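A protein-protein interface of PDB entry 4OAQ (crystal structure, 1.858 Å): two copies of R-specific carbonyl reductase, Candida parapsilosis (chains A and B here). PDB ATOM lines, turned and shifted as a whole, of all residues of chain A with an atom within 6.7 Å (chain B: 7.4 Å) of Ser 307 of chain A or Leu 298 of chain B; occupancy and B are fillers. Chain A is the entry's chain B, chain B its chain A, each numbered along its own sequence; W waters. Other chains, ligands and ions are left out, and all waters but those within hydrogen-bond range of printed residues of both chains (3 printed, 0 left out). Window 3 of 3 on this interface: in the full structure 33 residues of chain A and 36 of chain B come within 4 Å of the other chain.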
ATOM      1  N   GLN A 114      -5.666   1.026  29.541  1.00  0.00           N
ATOM      2  CA  GLN A 114      -6.409   0.967  28.289  1.00  0.00           C
ATOM      3  C   GLN A 114      -6.950  -0.446  28.093  1.00  0.00           C
ATOM      4  O   GLN A 114      -7.853  -0.676  27.290  1.00  0.00           O
ATOM      5  CB  GLN A 114      -5.534   1.391  27.099  1.00  0.00           C
ATOM      6  CG  GLN A 114      -4.451   0.389  26.685  1.00  0.00           C
ATOM      7  CD  GLN A 114      -3.137   0.558  27.441  1.00  0.00           C
ATOM      8  OE1 GLN A 114      -3.116   1.003  28.584  1.00  0.00           O
ATOM      9  NE2 GLN A 114      -2.029   0.188  26.797  1.00  0.00           N
ATOM     10  N   TYR A 115      -6.416  -1.382  28.863  1.00  0.00           N
ATOM     11  CA  TYR A 115      -6.882  -2.767  28.811  1.00  0.00           C
ATOM     12  C   TYR A 115      -7.744  -3.118  30.002  1.00  0.00           C
ATOM     13  O   TYR A 115      -8.090  -4.288  30.181  1.00  0.00           O
ATOM     14  CB  TYR A 115      -5.700  -3.739  28.752  1.00  0.00           C
ATOM     15  CG  TYR A 115      -4.954  -3.726  27.439  1.00  0.00           C
ATOM     16  CD1 TYR A 115      -5.462  -4.377  26.324  1.00  0.00           C
ATOM     17  CD2 TYR A 115      -3.724  -3.085  27.320  1.00  0.00           C
ATOM     18  CE1 TYR A 115      -4.772  -4.376  25.114  1.00  0.00           C
ATOM     19  CE2 TYR A 115      -3.028  -3.089  26.115  1.00  0.00           C
ATOM     20  CZ  TYR A 115      -3.556  -3.737  25.024  1.00  0.00           C
ATOM     21  OH  TYR A 115      -2.872  -3.728  23.817  1.00  0.00           O
ATOM     22  N   ILE A 170      -1.009   7.298  19.237  1.00  0.00           N
ATOM     23  CA  ILE A 170      -0.749   6.333  20.303  1.00  0.00           C
ATOM     24  C   ILE A 170      -0.977   4.895  19.855  1.00  0.00           C
ATOM     25  O   ILE A 170      -0.204   4.007  20.221  1.00  0.00           O
ATOM     26  CB  ILE A 170      -1.561   6.620  21.597  1.00  0.00           C
ATOM     27  CG1 ILE A 170      -1.151   5.662  22.716  1.00  0.00           C
ATOM     28  CG2 ILE A 170      -3.074   6.551  21.339  1.00  0.00           C
ATOM     29  CD1 ILE A 170       0.284   5.851  23.188  1.00  0.00           C
ATOM     30  N   THR A 171      -2.015   4.667  19.055  1.00  0.00           N
ATOM     31  CA  THR A 171      -2.309   3.326  18.557  1.00  0.00           C
ATOM     32  C   THR A 171      -1.123   2.769  17.788  1.00  0.00           C
ATOM     33  O   THR A 171      -0.854   1.575  17.881  1.00  0.00           O
ATOM     34  CB  THR A 171      -3.563   3.289  17.650  1.00  0.00           C
ATOM     35  OG1 THR A 171      -4.704   3.716  18.405  1.00  0.00           O
ATOM     36  CG2 THR A 171      -3.810   1.891  17.152  1.00  0.00           C
ATOM     37  N   SER A 174       2.449   2.895  20.636  1.00  0.00           N
ATOM     38  CA  SER A 174       2.473   1.894  21.696  1.00  0.00           C
ATOM     39  C   SER A 174       3.118   0.547  21.287  1.00  0.00           C
ATOM     40  O   SER A 174       4.072   0.099  21.940  1.00  0.00           O
ATOM     41  CB  SER A 174       1.058   1.710  22.272  1.00  0.00           C
ATOM     42  OG  SER A 174       1.036   0.705  23.269  1.00  0.00           O
ATOM     43  N   PRO A 175       2.631  -0.082  20.200  1.00  0.00           N
ATOM     44  CA  PRO A 175       3.263  -1.348  19.806  1.00  0.00           C
ATOM     45  C   PRO A 175       4.710  -1.152  19.368  1.00  0.00           C
ATOM     46  O   PRO A 175       5.513  -2.077  19.507  1.00  0.00           O
ATOM     47  CB  PRO A 175       2.414  -1.810  18.620  1.00  0.00           C
ATOM     48  CG  PRO A 175       1.775  -0.541  18.099  1.00  0.00           C
ATOM     49  CD  PRO A 175       1.494   0.252  19.320  1.00  0.00           C
ATOM     50  N   ARG A 178       6.719  -0.854  22.674  1.00  0.00           N
ATOM     51  CA  ARG A 178       6.614  -2.116  23.390  1.00  0.00           C
ATOM     52  C   ARG A 178       7.399  -3.224  22.727  1.00  0.00           C
ATOM     53  O   ARG A 178       7.831  -4.165  23.389  1.00  0.00           O
ATOM     54  CB  ARG A 178       5.142  -2.527  23.568  1.00  0.00           C
ATOM     55  CG  ARG A 178       4.395  -1.617  24.560  1.00  0.00           C
ATOM     56  CD  ARG A 178       3.062  -2.182  25.063  1.00  0.00           C
ATOM     57  NE  ARG A 178       2.509  -1.328  26.118  1.00  0.00           N
ATOM     58  CZ  ARG A 178       1.509  -1.656  26.936  1.00  0.00           C
ATOM     59  NH1 ARG A 178       0.915  -2.836  26.849  1.00  0.00           N
ATOM     60  NH2 ARG A 178       1.108  -0.792  27.857  1.00  0.00           N
ATOM     61  N   ASN A 179       7.590  -3.128  21.419  1.00  0.00           N
ATOM     62  CA  ASN A 179       8.255  -4.219  20.726  1.00  0.00           C
ATOM     63  C   ASN A 179       9.682  -3.892  20.273  1.00  0.00           C
ATOM     64  O   ASN A 179      10.535  -4.775  20.211  1.00  0.00           O
ATOM     65  CB  ASN A 179       7.381  -4.731  19.574  1.00  0.00           C
ATOM     66  CG  ASN A 179       6.174  -5.519  20.069  1.00  0.00           C
ATOM     67  OD1 ASN A 179       6.302  -6.679  20.483  1.00  0.00           O
ATOM     68  ND2 ASN A 179       5.002  -4.891  20.050  1.00  0.00           N
ATOM     69  N   LEU A 254       4.503  -4.285  11.817  1.00  0.00           N
ATOM     70  CA  LEU A 254       3.248  -3.720  12.281  1.00  0.00           C
ATOM     71  C   LEU A 254       2.313  -3.513  11.117  1.00  0.00           C
ATOM     72  O   LEU A 254       2.589  -2.731  10.210  1.00  0.00           O
ATOM     73  CB  LEU A 254       3.484  -2.405  13.023  1.00  0.00           C
ATOM     74  CG  LEU A 254       2.251  -1.698  13.619  1.00  0.00           C
ATOM     75  CD1 LEU A 254       1.682  -2.449  14.824  1.00  0.00           C
ATOM     76  CD2 LEU A 254       2.639  -0.303  14.014  1.00  0.00           C
ATOM     77  N   VAL A 279       2.231  -7.702  14.492  1.00  0.00           N
ATOM     78  CA  VAL A 279       1.118  -7.180  15.274  1.00  0.00           C
ATOM     79  C   VAL A 279       0.212  -6.344  14.409  1.00  0.00           C
ATOM     80  O   VAL A 279       0.700  -5.557  13.611  1.00  0.00           O
ATOM     81  CB  VAL A 279       1.649  -6.324  16.425  1.00  0.00           C
ATOM     82  CG1 VAL A 279       0.531  -5.460  17.031  1.00  0.00           C
ATOM     83  CG2 VAL A 279       2.270  -7.233  17.478  1.00  0.00           C
ATOM     84  N   SER A 280      -1.104  -6.487  14.569  1.00  0.00           N
ATOM     85  CA  SER A 280      -2.061  -5.707  13.790  1.00  0.00           C
ATOM     86  C   SER A 280      -2.782  -4.688  14.657  1.00  0.00           C
ATOM     87  O   SER A 280      -3.167  -5.004  15.779  1.00  0.00           O
ATOM     88  CB  SER A 280      -3.117  -6.611  13.142  1.00  0.00           C
ATOM     89  OG  SER A 280      -2.578  -7.335  12.046  1.00  0.00           O
ATOM     90  N   VAL A 281      -2.963  -3.473  14.136  1.00  0.00           N
ATOM     91  CA  VAL A 281      -3.758  -2.442  14.816  1.00  0.00           C
ATOM     92  C   VAL A 281      -4.825  -1.904  13.880  1.00  0.00           C
ATOM     93  O   VAL A 281      -4.739  -2.104  12.665  1.00  0.00           O
ATOM     94  CB  VAL A 281      -2.860  -1.264  15.335  1.00  0.00           C
ATOM     95  CG1 VAL A 281      -2.010  -1.719  16.482  1.00  0.00           C
ATOM     96  CG2 VAL A 281      -1.950  -0.709  14.210  1.00  0.00           C
ATOM     97  N   GLY A 282      -5.843  -1.252  14.440  1.00  0.00           N
ATOM     98  CA  GLY A 282      -6.877  -0.600  13.649  1.00  0.00           C
ATOM     99  C   GLY A 282      -7.856  -1.516  12.940  1.00  0.00           C
ATOM    100  O   GLY A 282      -8.601  -1.081  12.057  1.00  0.00           O
ATOM    101  N   LEU A 283      -7.864  -2.786  13.324  1.00  0.00           N
ATOM    102  CA  LEU A 283      -8.806  -3.732  12.743  1.00  0.00           C
ATOM    103  C   LEU A 283     -10.102  -3.709  13.547  1.00  0.00           C
ATOM    104  O   LEU A 283     -10.073  -3.580  14.772  1.00  0.00           O
ATOM    105  CB  LEU A 283      -8.208  -5.138  12.723  1.00  0.00           C
ATOM    106  CG  LEU A 283      -7.050  -5.344  11.740  1.00  0.00           C
ATOM    107  CD1 LEU A 283      -6.466  -6.749  11.845  1.00  0.00           C
ATOM    108  CD2 LEU A 283      -7.498  -5.042  10.306  1.00  0.00           C
ATOM    109  N   PRO A 284     -11.241  -3.812  12.859  1.00  0.00           N
ATOM    110  CA  PRO A 284     -12.529  -3.919  13.558  1.00  0.00           C
ATOM    111  C   PRO A 284     -12.524  -5.094  14.543  1.00  0.00           C
ATOM    112  O   PRO A 284     -12.043  -6.173  14.205  1.00  0.00           O
ATOM    113  CB  PRO A 284     -13.528  -4.186  12.423  1.00  0.00           C
ATOM    114  CG  PRO A 284     -12.682  -4.667  11.256  1.00  0.00           C
ATOM    115  CD  PRO A 284     -11.388  -3.931  11.400  1.00  0.00           C
ATOM    116  N   PRO A 285     -13.071  -4.891  15.747  1.00  0.00           N
ATOM    117  CA  PRO A 285     -13.051  -5.914  16.797  1.00  0.00           C
ATOM    118  C   PRO A 285     -14.097  -6.993  16.548  1.00  0.00           C
ATOM    119  O   PRO A 285     -14.937  -7.251  17.412  1.00  0.00           O
ATOM    120  CB  PRO A 285     -13.426  -5.119  18.042  1.00  0.00           C
ATOM    121  CG  PRO A 285     -14.393  -4.085  17.506  1.00  0.00           C
ATOM    122  CD  PRO A 285     -13.881  -3.720  16.131  1.00  0.00           C
ATOM    123  N   SER A 286     -14.037  -7.620  15.379  1.00  0.00           N
ATOM    124  CA  SER A 286     -14.996  -8.651  15.003  1.00  0.00           C
ATOM    125  C   SER A 286     -14.961  -9.860  15.937  1.00  0.00           C
ATOM    126  O   SER A 286     -13.894 -10.295  16.394  1.00  0.00           O
ATOM    127  CB  SER A 286     -14.733  -9.112  13.566  1.00  0.00           C
ATOM    128  OG  SER A 286     -15.666 -10.095  13.164  1.00  0.00           O
ATOM    129  N   GLY A 305      -0.342 -11.185  16.925  1.00  0.00           N
ATOM    130  CA  GLY A 305      -1.309 -10.667  17.879  1.00  0.00           C
ATOM    131  C   GLY A 305      -1.790  -9.267  17.567  1.00  0.00           C
ATOM    132  O   GLY A 305      -1.619  -8.762  16.451  1.00  0.00           O
ATOM    133  N   SER A 306      -2.406  -8.641  18.569  1.00  0.00           N
ATOM    134  CA  SER A 306      -2.991  -7.322  18.410  1.00  0.00           C
ATOM    135  C   SER A 306      -2.480  -6.350  19.458  1.00  0.00           C
ATOM    136  O   SER A 306      -1.818  -6.738  20.421  1.00  0.00           O
ATOM    137  CB  SER A 306      -4.513  -7.396  18.528  1.00  0.00           C
ATOM    138  OG  SER A 306      -5.100  -7.768  17.297  1.00  0.00           O
ATOM    139  N   SER A 307      -2.790  -5.075  19.256  1.00  0.00           N
ATOM    140  CA  SER A 307      -2.496  -4.056  20.249  1.00  0.00           C
ATOM    141  C   SER A 307      -3.676  -3.117  20.245  1.00  0.00           C
ATOM    142  O   SER A 307      -4.277  -2.893  19.197  1.00  0.00           O
ATOM    143  CB  SER A 307      -1.211  -3.293  19.907  1.00  0.00           C
ATOM    144  OG  SER A 307      -1.066  -2.166  20.768  1.00  0.00           O
ATOM    145  N   LEU A 308      -4.007  -2.592  21.419  1.00  0.00           N
ATOM    146  CA  LEU A 308      -5.141  -1.705  21.602  1.00  0.00           C
ATOM    147  C   LEU A 308      -4.601  -0.403  22.200  1.00  0.00           C
ATOM    148  O   LEU A 308      -3.975  -0.439  23.264  1.00  0.00           O
ATOM    149  CB  LEU A 308      -6.139  -2.355  22.577  1.00  0.00           C
ATOM    150  CG  LEU A 308      -7.630  -1.989  22.571  1.00  0.00           C
ATOM    151  CD1 LEU A 308      -8.155  -1.640  23.975  1.00  0.00           C
ATOM    152  CD2 LEU A 308      -7.948  -0.881  21.593  1.00  0.00           C
ATOM    153  N   LEU A 309      -4.808   0.717  21.499  1.00  0.00           N
ATOM    154  CA  LEU A 309      -4.431   2.059  21.963  1.00  0.00           C
ATOM    155  C   LEU A 309      -3.056   2.111  22.653  1.00  0.00           C
ATOM    156  O   LEU A 309      -2.080   1.591  22.118  1.00  0.00           O
ATOM    157  CB  LEU A 309      -5.510   2.620  22.898  1.00  0.00           C
ATOM    158  CG  LEU A 309      -6.944   2.571  22.365  1.00  0.00           C
ATOM    159  CD1 LEU A 309      -7.948   3.126  23.386  1.00  0.00           C
ATOM    160  CD2 LEU A 309      -7.042   3.346  21.050  1.00  0.00           C
ATOM    161  N   GLY A 310      -2.988   2.741  23.828  1.00  0.00           N
ATOM    162  CA  GLY A 310      -1.748   2.809  24.591  1.00  0.00           C
ATOM    163  C   GLY A 310      -1.931   3.462  25.952  1.00  0.00           C
ATOM    164  O   GLY A 310      -3.020   3.905  26.290  1.00  0.00           O
ATOM    165  N   ASP B 275      -0.033  -8.411  26.867  1.00  0.00           N
ATOM    166  CA  ASP B 275       1.163  -8.537  26.034  1.00  0.00           C
ATOM    167  C   ASP B 275       2.002  -9.771  26.316  1.00  0.00           C
ATOM    168  O   ASP B 275       3.224  -9.739  26.177  1.00  0.00           O
ATOM    169  CB  ASP B 275       2.041  -7.298  26.171  1.00  0.00           C
ATOM    170  CG  ASP B 275       1.605  -6.191  25.269  1.00  0.00           C
ATOM    171  OD1 ASP B 275       0.451  -6.244  24.796  1.00  0.00           O
ATOM    172  OD2 ASP B 275       2.417  -5.278  25.026  1.00  0.00           O
ATOM    173  N   SER B 293     -11.201 -15.194  17.677  1.00  0.00           N
ATOM    174  CA  SER B 293     -11.598 -13.915  17.064  1.00  0.00           C
ATOM    175  C   SER B 293     -10.650 -12.742  17.353  1.00  0.00           C
ATOM    176  O   SER B 293      -9.965 -12.737  18.372  1.00  0.00           O
ATOM    177  CB  SER B 293     -13.001 -13.526  17.540  1.00  0.00           C
ATOM    178  OG  SER B 293     -12.968 -13.154  18.908  1.00  0.00           O
ATOM    179  N   PRO B 294     -10.630 -11.733  16.459  1.00  0.00           N
ATOM    180  CA  PRO B 294      -9.872 -10.492  16.681  1.00  0.00           C
ATOM    181  C   PRO B 294     -10.173  -9.860  18.045  1.00  0.00           C
ATOM    182  O   PRO B 294      -9.287  -9.249  18.669  1.00  0.00           O
ATOM    183  CB  PRO B 294     -10.377  -9.572  15.563  1.00  0.00           C
ATOM    184  CG  PRO B 294     -10.776 -10.497  14.468  1.00  0.00           C
ATOM    185  CD  PRO B 294     -11.288 -11.749  15.137  1.00  0.00           C
ATOM    186  N   PHE B 295     -11.421 -10.017  18.486  1.00  0.00           N
ATOM    187  CA  PHE B 295     -11.880  -9.547  19.786  1.00  0.00           C
ATOM    188  C   PHE B 295     -10.958 -10.007  20.902  1.00  0.00           C
ATOM    189  O   PHE B 295     -10.364  -9.195  21.626  1.00  0.00           O
ATOM    190  CB  PHE B 295     -13.297 -10.066  20.045  1.00  0.00           C
ATOM    191  CG  PHE B 295     -13.860  -9.680  21.384  1.00  0.00           C
ATOM    192  CD1 PHE B 295     -14.580  -8.506  21.531  1.00  0.00           C
ATOM    193  CD2 PHE B 295     -13.693 -10.505  22.489  1.00  0.00           C
ATOM    194  CE1 PHE B 295     -15.111  -8.148  22.760  1.00  0.00           C
ATOM    195  CE2 PHE B 295     -14.223 -10.154  23.719  1.00  0.00           C
ATOM    196  CZ  PHE B 295     -14.931  -8.974  23.855  1.00  0.00           C
ATOM    197  N   THR B 296     -10.830 -11.316  21.047  1.00  0.00           N
ATOM    198  CA  THR B 296     -10.124 -11.822  22.208  1.00  0.00           C
ATOM    199  C   THR B 296      -8.616 -11.554  22.140  1.00  0.00           C
ATOM    200  O   THR B 296      -7.960 -11.470  23.174  1.00  0.00           O
ATOM    201  CB  THR B 296     -10.475 -13.303  22.525  1.00  0.00           C
ATOM    202  OG1 THR B 296     -10.013 -13.637  23.843  1.00  0.00           O
ATOM    203  CG2 THR B 296      -9.869 -14.242  21.513  1.00  0.00           C
ATOM    204  N   PHE B 297      -8.064 -11.400  20.941  1.00  0.00           N
ATOM    205  CA  PHE B 297      -6.688 -10.908  20.844  1.00  0.00           C
ATOM    206  C   PHE B 297      -6.658  -9.494  21.403  1.00  0.00           C
ATOM    207  O   PHE B 297      -5.751  -9.128  22.143  1.00  0.00           O
ATOM    208  CB  PHE B 297      -6.190 -10.869  19.399  1.00  0.00           C
ATOM    209  CG  PHE B 297      -5.663 -12.170  18.901  1.00  0.00           C
ATOM    210  CD1 PHE B 297      -4.532 -12.731  19.460  1.00  0.00           C
ATOM    211  CD2 PHE B 297      -6.281 -12.815  17.845  1.00  0.00           C
ATOM    212  CE1 PHE B 297      -4.043 -13.938  18.990  1.00  0.00           C
ATOM    213  CE2 PHE B 297      -5.803 -14.017  17.372  1.00  0.00           C
ATOM    214  CZ  PHE B 297      -4.680 -14.582  17.946  1.00  0.00           C
ATOM    215  N   LEU B 298      -7.660  -8.703  21.041  1.00  0.00           N
ATOM    216  CA  LEU B 298      -7.693  -7.302  21.434  1.00  0.00           C
ATOM    217  C   LEU B 298      -7.855  -7.086  22.932  1.00  0.00           C
ATOM    218  O   LEU B 298      -7.375  -6.084  23.462  1.00  0.00           O
ATOM    219  CB  LEU B 298      -8.792  -6.551  20.681  1.00  0.00           C
ATOM    220  CG  LEU B 298      -8.392  -6.001  19.314  1.00  0.00           C
ATOM    221  CD1 LEU B 298      -9.584  -5.346  18.608  1.00  0.00           C
ATOM    222  CD2 LEU B 298      -7.254  -5.004  19.486  1.00  0.00           C
ATOM    223  N   GLN B 299      -8.544  -7.998  23.616  1.00  0.00           N
ATOM    224  CA  GLN B 299      -8.796  -7.796  25.044  1.00  0.00           C
ATOM    225  C   GLN B 299      -7.510  -7.701  25.873  1.00  0.00           C
ATOM    226  O   GLN B 299      -7.476  -6.972  26.863  1.00  0.00           O
ATOM    227  CB  GLN B 299      -9.711  -8.887  25.617  1.00  0.00           C
ATOM    228  CG  GLN B 299     -10.923  -9.244  24.763  1.00  0.00           C
ATOM    229  CD  GLN B 299     -11.725  -8.034  24.304  1.00  0.00           C
ATOM    230  OE1 GLN B 299     -12.397  -7.368  25.100  1.00  0.00           O
ATOM    231  NE2 GLN B 299     -11.666  -7.752  23.007  1.00  0.00           N
ATOM    232  N   GLN B 300      -6.458  -8.393  25.434  1.00  0.00           N
ATOM    233  CA  GLN B 300      -5.249  -8.623  26.227  1.00  0.00           C
ATOM    234  C   GLN B 300      -3.934  -8.173  25.578  1.00  0.00           C
ATOM    235  O   GLN B 300      -2.882  -8.223  26.224  1.00  0.00           O
ATOM    236  CB  GLN B 300      -5.088 -10.136  26.452  1.00  0.00           C
ATOM    237  CG  GLN B 300      -5.380 -10.625  27.842  1.00  0.00           C
ATOM    238  CD  GLN B 300      -6.840 -10.513  28.213  1.00  0.00           C
ATOM    239  OE1 GLN B 300      -7.185  -9.950  29.249  1.00  0.00           O
ATOM    240  NE2 GLN B 300      -7.709 -11.065  27.375  1.00  0.00           N
ATOM    241  N   GLY B 301      -3.969  -7.823  24.296  1.00  0.00           N
ATOM    242  CA  GLY B 301      -2.741  -7.723  23.519  1.00  0.00           C
ATOM    243  C   GLY B 301      -1.981  -9.038  23.525  1.00  0.00           C
ATOM    244  O   GLY B 301      -0.753  -9.077  23.449  1.00  0.00           O
ATOM    245  N   ALA B 302      -2.722 -10.135  23.613  1.00  0.00           N
ATOM    246  CA  ALA B 302      -2.121 -11.455  23.675  1.00  0.00           C
ATOM    247  C   ALA B 302      -1.643 -11.880  22.306  1.00  0.00           C
ATOM    248  O   ALA B 302      -2.240 -11.528  21.299  1.00  0.00           O
ATOM    249  CB  ALA B 302      -3.124 -12.451  24.186  1.00  0.00           C
HETATM  250  O   HOH W   1      -0.178  -3.738  24.034  1.00  0.00           O
HETATM  251  O   HOH W   2      -9.685  -5.547  28.116  1.00  0.00           O
HETATM  252  O   HOH W   3       0.291  -8.624  20.537  1.00  0.00           O
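N of Phe 295 of chain B sits at hydrogen-bond distance from O of Ser 286 of chain A (3.3 Å).
The side-chain carboxylate (OD2) of Asp 275 of chain B lies within salt-bridge range of the guanidinium group (NH1) of Arg 178 of chain A.
N of Ser 280 of chain A sits at hydrogen-bond distance from O of Gly 305 of chain A (3.0 Å).
NE2 of Gln 114 of chain A lies close to NH2 of Arg 178 of chain A (3.5 Å).
N of Asp 275 of chain B is in hydrogen-bond range of O of Gln 300 of chain B (2.9 Å).
The side-chain hydroxyl (OH) of Tyr 115 of chain A sits at hydrogen-bond distance from the backbone NH (N) of Leu 308 of chain A.
The backbone carbonyl oxygen of Ser 280 of chain A sits at hydrogen-bond distance from the backbone NH of Ser 307 of chain A, at 3.5 Å.
CD1 of Tyr 115 of chain A touches O of Gln 299 of chain B (3.3 Å).
N of Gly 301 of chain B touches CE1 of Tyr 115 of chain A, at 3.6 Å.
Pro 285 of chain A touches Leu 298 of chain B (CB to CD1, 3.9 Å).
CB of Ser 293 of chain B touches O of Ser 286 of chain A, 3.5 Å away.
Ser 286 of chain A touches Pro 294 of chain B.
OG of Ser 306 of chain A touches CB of Phe 297 of chain B, at 3.9 Å.
Ser 306 of chain A touches Leu 298 of chain B.
CA of Gly 301 of chain B touches O of Ser 306 of chain A (3.4 Å).
Ser 306 of chain A touches Ala 302 of chain B.
O of Ser 307 of chain A touches CD2 of Leu 298 of chain B, at 3.7 Å.
Of the printed residues of chain B, Pro 285 of chain A touches Leu 298.
Printed residues of chain B within 4 Å of Gly 305 of chain A: Ala 302.
Of chain B, only Leu 298 (3.7 Å) comes within 4 Å of Ser 307 of chain A.
Of the printed residues of chain A, Ser 293 of chain B touches Ser 286 (3.5 Å).
Of the printed residues of chain A, Phe 297 of chain B touches Ser 306 (3.9 Å).
Printed residues of chain A within 4 Å of Leu 298 of chain B: Tyr 115 (3.5 Å), Pro 285 (3.9 Å), Ser 306 (3.8 Å) and Ser 307 (3.7 Å).
Of the printed residues of chain A, Gln 300 of chain B touches Tyr 115.
Printed residues of chain A that touch a printed residue of chain B: Tyr 115, Arg 178, Pro 285, Ser 286, Gly 305, Ser 306 and Ser 307.
Of the 11 printed residues of chain B, 10 touch a printed residue of chain A.
Among the printed residues, 15 pairs touch across the chains.
Among the printed residues, Asp or Glu carboxylates within 4 Å of a Lys or Arg side-chain nitrogen of the other chain: Arg 178 of chain A with Asp 275 of chain B (3.4 Å).
No position is printed for both chains.
Water W1 lies within hydrogen-bond range of the side-chain carboxylate of Asp 275 of chain B, the side-chain hydroxyl of Tyr 115 of chain A and the guanidinium group of Arg 178 of chain A.
Water W3 bridges O of Ser 306 of chain A (2.8 Å) and O of Gly 301 of chain B (3.1 Å).
Water W2 lies within hydrogen-bond range of the backbone carbonyl oxygen (O) of Tyr 115 of chain A (2.9 Å) and the backbone carbonyl oxygen (O) of Gln 299 of chain B (2.9 Å).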
